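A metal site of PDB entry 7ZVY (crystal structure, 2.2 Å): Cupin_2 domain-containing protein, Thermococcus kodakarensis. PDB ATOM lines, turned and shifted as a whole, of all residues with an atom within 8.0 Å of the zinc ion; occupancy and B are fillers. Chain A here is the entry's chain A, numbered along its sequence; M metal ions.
The side-chain carboxylate of Glu 51 sits close to the side-chain amide oxygen of Gln 49, 3.4 Å away. A ring nitrogen (ND1) of His 44 is in hydrogen-bond range of the backbone carbonyl oxygen of Lys 42 (2.8 Å). The backbone NH (N) of Val 79 lies within hydrogen-bond range of the backbone carbonyl oxygen (O) of Glu 51. The backbone NH (N) of His 44 is in hydrogen-bond range of the backbone carbonyl oxygen (O) of His 85.
Merely in contact with the zinc ion: His 44. Of the 23 residues printed, 4 come within 4 Å of the zinc ion.
The zinc ion is bound by the side-chain carboxylate (OE1) of Glu 51, a ring nitrogen (NE2) of His 46, a ring nitrogen (NE2) of His 85 and the side-chain carboxylate (OE2) of Glu 51. The zinc ion has four donor atoms within binding distance.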
ATOM      1  N   TYR A  14     -26.114 -37.864  27.391  1.00  0.00           N
ATOM      2  CA  TYR A  14     -27.380 -37.147  27.108  1.00  0.00           C
ATOM      3  C   TYR A  14     -27.566 -36.959  25.610  1.00  0.00           C
ATOM      4  O   TYR A  14     -26.831 -37.601  24.827  1.00  0.00           O
ATOM      5  CB  TYR A  14     -27.353 -35.772  27.797  1.00  0.00           C
ATOM      6  CG  TYR A  14     -26.231 -34.881  27.327  1.00  0.00           C
ATOM      7  CD1 TYR A  14     -24.959 -34.982  27.860  1.00  0.00           C
ATOM      8  CD2 TYR A  14     -26.445 -33.938  26.331  1.00  0.00           C
ATOM      9  CE1 TYR A  14     -23.923 -34.169  27.433  1.00  0.00           C
ATOM     10  CE2 TYR A  14     -25.414 -33.117  25.893  1.00  0.00           C
ATOM     11  CZ  TYR A  14     -24.153 -33.231  26.451  1.00  0.00           C
ATOM     12  OH  TYR A  14     -23.141 -32.423  26.023  1.00  0.00           O
ATOM     13  N   GLN A  31     -32.392 -25.166  21.786  1.00  0.00           N
ATOM     14  CA  GLN A  31     -32.316 -26.605  21.690  1.00  0.00           C
ATOM     15  C   GLN A  31     -32.910 -27.133  22.957  1.00  0.00           C
ATOM     16  O   GLN A  31     -33.034 -26.358  23.909  1.00  0.00           O
ATOM     17  CB  GLN A  31     -30.855 -26.993  21.565  1.00  0.00           C
ATOM     18  CG  GLN A  31     -30.254 -27.075  22.937  1.00  0.00           C
ATOM     19  CD  GLN A  31     -28.758 -27.134  22.853  1.00  0.00           C
ATOM     20  OE1 GLN A  31     -28.096 -26.846  21.878  1.00  0.00           O
ATOM     21  NE2 GLN A  31     -28.231 -27.606  23.953  1.00  0.00           N
ATOM     22  N   VAL A  33     -32.665 -30.306  25.677  1.00  0.00           N
ATOM     23  CA  VAL A  33     -31.550 -31.129  26.189  1.00  0.00           C
ATOM     24  C   VAL A  33     -32.213 -32.189  27.004  1.00  0.00           C
ATOM     25  O   VAL A  33     -33.146 -31.916  27.799  1.00  0.00           O
ATOM     26  CB  VAL A  33     -30.526 -30.385  27.040  1.00  0.00           C
ATOM     27  CG1 VAL A  33     -29.466 -31.337  27.606  1.00  0.00           C
ATOM     28  CG2 VAL A  33     -29.913 -29.299  26.204  1.00  0.00           C
ATOM     29  N   VAL A  41     -24.251 -35.151  33.701  1.00  0.00           N
ATOM     30  CA  VAL A  41     -23.455 -34.314  32.780  1.00  0.00           C
ATOM     31  C   VAL A  41     -22.330 -33.741  33.611  1.00  0.00           C
ATOM     32  O   VAL A  41     -22.655 -33.111  34.606  1.00  0.00           O
ATOM     33  CB  VAL A  41     -24.379 -33.245  32.165  1.00  0.00           C
ATOM     34  CG1 VAL A  41     -23.541 -32.223  31.432  1.00  0.00           C
ATOM     35  CG2 VAL A  41     -25.362 -33.897  31.247  1.00  0.00           C
ATOM     36  N   LYS A  42     -21.069 -34.022  33.247  1.00  0.00           N
ATOM     37  CA  LYS A  42     -19.820 -33.786  34.042  1.00  0.00           C
ATOM     38  C   LYS A  42     -19.520 -32.289  34.045  1.00  0.00           C
ATOM     39  O   LYS A  42     -19.838 -31.624  33.052  1.00  0.00           O
ATOM     40  CB  LYS A  42     -18.592 -34.459  33.412  1.00  0.00           C
ATOM     41  CG  LYS A  42     -18.601 -36.004  33.404  1.00  0.00           C
ATOM     42  CD  LYS A  42     -17.371 -36.661  32.747  1.00  0.00           C
ATOM     43  CE  LYS A  42     -17.372 -38.173  32.760  1.00  0.00           C
ATOM     44  NZ  LYS A  42     -16.170 -38.717  32.089  1.00  0.00           N
ATOM     45  N   HIS A  44     -18.427 -28.580  33.657  1.00  0.00           N
ATOM     46  CA  HIS A  44     -18.003 -27.926  32.394  1.00  0.00           C
ATOM     47  C   HIS A  44     -18.351 -26.434  32.422  1.00  0.00           C
ATOM     48  O   HIS A  44     -19.290 -26.054  33.148  1.00  0.00           O
ATOM     49  CB  HIS A  44     -18.630 -28.630  31.182  1.00  0.00           C
ATOM     50  CG  HIS A  44     -20.118 -28.628  31.180  1.00  0.00           C
ATOM     51  ND1 HIS A  44     -20.863 -29.213  32.181  1.00  0.00           N
ATOM     52  CD2 HIS A  44     -21.011 -28.115  30.302  1.00  0.00           C
ATOM     53  CE1 HIS A  44     -22.147 -29.061  31.935  1.00  0.00           C
ATOM     54  NE2 HIS A  44     -22.261 -28.395  30.779  1.00  0.00           N
ATOM     55  N   TYR A  45     -17.610 -25.624  31.644  1.00  0.00           N
ATOM     56  CA  TYR A  45     -17.833 -24.155  31.619  1.00  0.00           C
ATOM     57  C   TYR A  45     -17.831 -23.669  30.166  1.00  0.00           C
ATOM     58  O   TYR A  45     -17.220 -24.336  29.302  1.00  0.00           O
ATOM     59  CB  TYR A  45     -16.761 -23.436  32.453  1.00  0.00           C
ATOM     60  CG  TYR A  45     -15.766 -22.640  31.649  1.00  0.00           C
ATOM     61  CD1 TYR A  45     -16.013 -21.321  31.317  1.00  0.00           C
ATOM     62  CD2 TYR A  45     -14.583 -23.202  31.225  1.00  0.00           C
ATOM     63  CE1 TYR A  45     -15.111 -20.574  30.590  1.00  0.00           C
ATOM     64  CE2 TYR A  45     -13.662 -22.466  30.489  1.00  0.00           C
ATOM     65  CZ  TYR A  45     -13.926 -21.153  30.171  1.00  0.00           C
ATOM     66  OH  TYR A  45     -13.029 -20.418  29.448  1.00  0.00           O
ATOM     67  N   HIS A  46     -18.478 -22.532  29.902  1.00  0.00           N
ATOM     68  CA  HIS A  46     -18.582 -22.031  28.507  1.00  0.00           C
ATOM     69  C   HIS A  46     -17.711 -20.778  28.332  1.00  0.00           C
ATOM     70  O   HIS A  46     -17.871 -19.845  29.145  1.00  0.00           O
ATOM     71  CB  HIS A  46     -20.054 -21.777  28.158  1.00  0.00           C
ATOM     72  CG  HIS A  46     -20.857 -23.039  28.165  1.00  0.00           C
ATOM     73  ND1 HIS A  46     -20.330 -24.243  27.724  1.00  0.00           N
ATOM     74  CD2 HIS A  46     -22.110 -23.297  28.591  1.00  0.00           C
ATOM     75  CE1 HIS A  46     -21.242 -25.184  27.861  1.00  0.00           C
ATOM     76  NE2 HIS A  46     -22.343 -24.635  28.387  1.00  0.00           N
ATOM     77  N   GLN A  49     -20.337 -18.158  26.052  1.00  0.00           N
ATOM     78  CA  GLN A  49     -21.799 -18.153  25.748  1.00  0.00           C
ATOM     79  C   GLN A  49     -22.552 -18.172  27.064  1.00  0.00           C
ATOM     80  O   GLN A  49     -22.015 -18.693  28.083  1.00  0.00           O
ATOM     81  CB  GLN A  49     -22.217 -19.291  24.828  1.00  0.00           C
ATOM     82  CG  GLN A  49     -22.650 -20.503  25.616  1.00  0.00           C
ATOM     83  CD  GLN A  49     -22.424 -21.797  24.887  1.00  0.00           C
ATOM     84  OE1 GLN A  49     -22.782 -22.878  25.342  1.00  0.00           O
ATOM     85  NE2 GLN A  49     -21.820 -21.682  23.712  1.00  0.00           N
ATOM     86  N   TYR A  50     -23.723 -17.583  27.058  1.00  0.00           N
ATOM     87  CA  TYR A  50     -24.638 -17.687  28.210  1.00  0.00           C
ATOM     88  C   TYR A  50     -25.626 -18.797  27.900  1.00  0.00           C
ATOM     89  O   TYR A  50     -25.924 -18.996  26.732  1.00  0.00           O
ATOM     90  CB  TYR A  50     -25.371 -16.389  28.512  1.00  0.00           C
ATOM     91  CG  TYR A  50     -24.487 -15.257  28.982  1.00  0.00           C
ATOM     92  CD1 TYR A  50     -24.789 -14.578  30.157  1.00  0.00           C
ATOM     93  CD2 TYR A  50     -23.417 -14.817  28.231  1.00  0.00           C
ATOM     94  CE1 TYR A  50     -24.031 -13.500  30.592  1.00  0.00           C
ATOM     95  CE2 TYR A  50     -22.648 -13.747  28.654  1.00  0.00           C
ATOM     96  CZ  TYR A  50     -22.944 -13.100  29.840  1.00  0.00           C
ATOM     97  OH  TYR A  50     -22.173 -12.054  30.263  1.00  0.00           O
ATOM     98  N   GLU A  51     -26.102 -19.469  28.926  1.00  0.00           N
ATOM     99  CA  GLU A  51     -27.078 -20.550  28.757  1.00  0.00           C
ATOM    100  C   GLU A  51     -28.273 -20.223  29.633  1.00  0.00           C
ATOM    101  O   GLU A  51     -28.108 -20.275  30.889  1.00  0.00           O
ATOM    102  CB  GLU A  51     -26.440 -21.900  29.111  1.00  0.00           C
ATOM    103  CG  GLU A  51     -25.689 -22.531  27.942  1.00  0.00           C
ATOM    104  CD  GLU A  51     -25.350 -24.000  28.187  1.00  0.00           C
ATOM    105  OE1 GLU A  51     -25.485 -24.429  29.357  1.00  0.00           O
ATOM    106  OE2 GLU A  51     -24.902 -24.723  27.211  1.00  0.00           O
ATOM    107  N   PHE A  53     -31.659 -21.758  30.886  1.00  0.00           N
ATOM    108  CA  PHE A  53     -32.385 -23.022  31.035  1.00  0.00           C
ATOM    109  C   PHE A  53     -33.823 -22.745  31.440  1.00  0.00           C
ATOM    110  O   PHE A  53     -34.082 -22.046  32.415  1.00  0.00           O
ATOM    111  CB  PHE A  53     -31.800 -23.921  32.134  1.00  0.00           C
ATOM    112  CG  PHE A  53     -30.344 -24.325  31.998  1.00  0.00           C
ATOM    113  CD1 PHE A  53     -29.691 -24.195  30.780  1.00  0.00           C
ATOM    114  CD2 PHE A  53     -29.630 -24.797  33.097  1.00  0.00           C
ATOM    115  CE1 PHE A  53     -28.334 -24.510  30.659  1.00  0.00           C
ATOM    116  CE2 PHE A  53     -28.276 -25.116  32.984  1.00  0.00           C
ATOM    117  CZ  PHE A  53     -27.635 -24.991  31.759  1.00  0.00           C
ATOM    118  N   VAL A  79     -26.398 -19.565  33.211  1.00  0.00           N
ATOM    119  CA  VAL A  79     -24.998 -19.973  33.508  1.00  0.00           C
ATOM    120  C   VAL A  79     -24.042 -18.971  32.853  1.00  0.00           C
ATOM    121  O   VAL A  79     -23.668 -19.198  31.642  1.00  0.00           O
ATOM    122  CB  VAL A  79     -24.659 -21.407  33.046  1.00  0.00           C
ATOM    123  CG1 VAL A  79     -23.250 -21.738  33.484  1.00  0.00           C
ATOM    124  CG2 VAL A  79     -25.674 -22.403  33.581  1.00  0.00           C
ATOM    125  N   THR A  83     -18.370 -19.946  34.210  1.00  0.00           N
ATOM    126  CA  THR A  83     -19.130 -20.561  35.321  1.00  0.00           C
ATOM    127  C   THR A  83     -19.222 -22.089  35.128  1.00  0.00           C
ATOM    128  O   THR A  83     -19.690 -22.550  34.041  1.00  0.00           O
ATOM    129  CB  THR A  83     -20.533 -19.975  35.454  1.00  0.00           C
ATOM    130  OG1 THR A  83     -20.483 -18.534  35.437  1.00  0.00           O
ATOM    131  CG2 THR A  83     -21.184 -20.440  36.741  1.00  0.00           C
ATOM    132  N   HIS A  85     -20.626 -25.685  35.582  1.00  0.00           N
ATOM    133  CA  HIS A  85     -21.914 -26.357  35.814  1.00  0.00           C
ATOM    134  C   HIS A  85     -21.858 -27.828  35.414  1.00  0.00           C
ATOM    135  O   HIS A  85     -20.877 -28.267  34.784  1.00  0.00           O
ATOM    136  CB  HIS A  85     -23.044 -25.583  35.137  1.00  0.00           C
ATOM    137  CG  HIS A  85     -22.970 -25.539  33.643  1.00  0.00           C
ATOM    138  ND1 HIS A  85     -22.386 -24.504  32.937  1.00  0.00           N
ATOM    139  CD2 HIS A  85     -23.640 -26.321  32.723  1.00  0.00           C
ATOM    140  CE1 HIS A  85     -22.566 -24.702  31.642  1.00  0.00           C
ATOM    141  NE2 HIS A  85     -23.314 -25.813  31.485  1.00  0.00           N
ATOM    142  N   TRP A  86     -22.913 -28.527  35.880  1.00  0.00           N
ATOM    143  CA  TRP A  86     -23.048 -29.987  35.752  1.00  0.00           C
ATOM    144  C   TRP A  86     -24.412 -30.431  36.287  1.00  0.00           C
ATOM    145  O   TRP A  86     -25.071 -29.622  36.985  1.00  0.00           O
ATOM    146  CB  TRP A  86     -22.007 -30.648  36.631  1.00  0.00           C
ATOM    147  CG  TRP A  86     -22.310 -30.456  38.097  1.00  0.00           C
ATOM    148  CD1 TRP A  86     -23.214 -31.114  38.894  1.00  0.00           C
ATOM    149  CD2 TRP A  86     -21.706 -29.448  38.936  1.00  0.00           C
ATOM    150  NE1 TRP A  86     -23.192 -30.584  40.171  1.00  0.00           N
ATOM    151  CE2 TRP A  86     -22.248 -29.585  40.235  1.00  0.00           C
ATOM    152  CE3 TRP A  86     -20.708 -28.479  38.718  1.00  0.00           C
ATOM    153  CZ2 TRP A  86     -21.826 -28.767  41.294  1.00  0.00           C
ATOM    154  CZ3 TRP A  86     -20.327 -27.662  39.758  1.00  0.00           C
ATOM    155  CH2 TRP A  86     -20.892 -27.788  41.029  1.00  0.00           C
ATOM    156  N   LEU A  97     -34.834 -30.009  29.351  1.00  0.00           N
ATOM    157  CA  LEU A  97     -34.848 -28.552  29.545  1.00  0.00           C
ATOM    158  C   LEU A  97     -34.684 -27.839  28.221  1.00  0.00           C
ATOM    159  O   LEU A  97     -33.970 -28.342  27.343  1.00  0.00           O
ATOM    160  CB  LEU A  97     -33.740 -28.127  30.521  1.00  0.00           C
ATOM    161  CG  LEU A  97     -32.384 -28.781  30.381  1.00  0.00           C
ATOM    162  CD1 LEU A  97     -31.316 -27.812  30.860  1.00  0.00           C
ATOM    163  CD2 LEU A  97     -32.338 -30.058  31.227  1.00  0.00           C
ATOM    164  N   VAL A  99     -33.158 -24.839  26.325  1.00  0.00           N
ATOM    165  CA  VAL A  99     -31.946 -24.059  26.564  1.00  0.00           C
ATOM    166  C   VAL A  99     -31.953 -23.036  25.434  1.00  0.00           C
ATOM    167  O   VAL A  99     -32.415 -23.329  24.328  1.00  0.00           O
ATOM    168  CB  VAL A  99     -30.699 -25.004  26.623  1.00  0.00           C
ATOM    169  CG1 VAL A  99     -29.400 -24.248  26.730  1.00  0.00           C
ATOM    170  CG2 VAL A  99     -30.824 -26.045  27.722  1.00  0.00           C
ATOM    171  N   LYS A 101     -28.776 -20.341  24.025  1.00  0.00           N
ATOM    172  CA  LYS A 101     -27.381 -19.899  24.265  1.00  0.00           C
ATOM    173  C   LYS A 101     -27.239 -18.444  23.825  1.00  0.00           C
ATOM    174  O   LYS A 101     -27.722 -18.113  22.718  1.00  0.00           O
ATOM    175  CB  LYS A 101     -26.403 -20.800  23.503  1.00  0.00           C
ATOM    176  CG  LYS A 101     -26.969 -22.155  23.082  1.00  0.00           C
ATOM    177  CD  LYS A 101     -25.907 -23.119  22.614  1.00  0.00           C
ATOM    178  CE  LYS A 101     -26.177 -24.543  23.039  1.00  0.00           C
ATOM    179  NZ  LYS A 101     -25.677 -25.513  22.029  1.00  0.00           N
ATOM    180  N   ASP A 108     -18.184 -22.813  22.504  1.00  0.00           N
ATOM    181  CA  ASP A 108     -17.316 -22.215  23.536  1.00  0.00           C
ATOM    182  C   ASP A 108     -17.242 -23.186  24.710  1.00  0.00           C
ATOM    183  O   ASP A 108     -16.583 -22.876  25.707  1.00  0.00           O
ATOM    184  CB  ASP A 108     -17.851 -20.852  23.959  1.00  0.00           C
ATOM    185  CG  ASP A 108     -18.915 -20.962  25.030  1.00  0.00           C
ATOM    186  OD1 ASP A 108     -19.663 -21.956  25.031  1.00  0.00           O
ATOM    187  OD2 ASP A 108     -18.968 -20.070  25.882  1.00  0.00           O
ATOM    188  N   SER A 109     -17.948 -24.317  24.623  1.00  0.00           N
ATOM    189  CA  SER A 109     -18.036 -25.230  25.791  1.00  0.00           C
ATOM    190  C   SER A 109     -16.672 -25.808  26.178  1.00  0.00           C
ATOM    191  O   SER A 109     -15.902 -26.170  25.265  1.00  0.00           O
ATOM    192  CB  SER A 109     -19.022 -26.339  25.518  1.00  0.00           C
ATOM    193  OG  SER A 109     -18.442 -27.335  24.689  1.00  0.00           O
ATOM    194  N   VAL A 110     -16.395 -25.884  27.483  1.00  0.00           N
ATOM    195  CA  VAL A 110     -15.134 -26.513  27.992  1.00  0.00           C
ATOM    196  C   VAL A 110     -15.543 -27.383  29.187  1.00  0.00           C
ATOM    197  O   VAL A 110     -16.537 -27.022  29.831  1.00  0.00           O
ATOM    198  CB  VAL A 110     -14.091 -25.442  28.379  1.00  0.00           C
ATOM    199  CG1 VAL A 110     -13.245 -25.868  29.560  1.00  0.00           C
ATOM    200  CG2 VAL A 110     -13.213 -25.066  27.195  1.00  0.00           C
ATOM    201  N   TRP A 111     -14.836 -28.472  29.466  1.00  0.00           N
ATOM    202  CA  TRP A 111     -15.284 -29.389  30.559  1.00  0.00           C
ATOM    203  C   TRP A 111     -14.153 -29.658  31.548  1.00  0.00           C
ATOM    204  O   TRP A 111     -13.036 -29.989  31.094  1.00  0.00           O
ATOM    205  CB  TRP A 111     -15.828 -30.689  29.946  1.00  0.00           C
ATOM    206  CG  TRP A 111     -17.063 -30.499  29.124  1.00  0.00           C
ATOM    207  CD1 TRP A 111     -17.213 -29.699  28.021  1.00  0.00           C
ATOM    208  CD2 TRP A 111     -18.344 -31.117  29.327  1.00  0.00           C
ATOM    209  NE1 TRP A 111     -18.490 -29.775  27.539  1.00  0.00           N
ATOM    210  CE2 TRP A 111     -19.208 -30.632  28.326  1.00  0.00           C
ATOM    211  CE3 TRP A 111     -18.851 -32.019  30.268  1.00  0.00           C
ATOM    212  CZ2 TRP A 111     -20.539 -31.030  28.221  1.00  0.00           C
ATOM    213  CZ3 TRP A 111     -20.171 -32.413  30.171  1.00  0.00           C
ATOM    214  CH2 TRP A 111     -20.998 -31.922  29.165  1.00  0.00           C
HETATM  215 ZN    ZN M   1     -24.028 -26.263  29.085  1.00  0.00          ZN
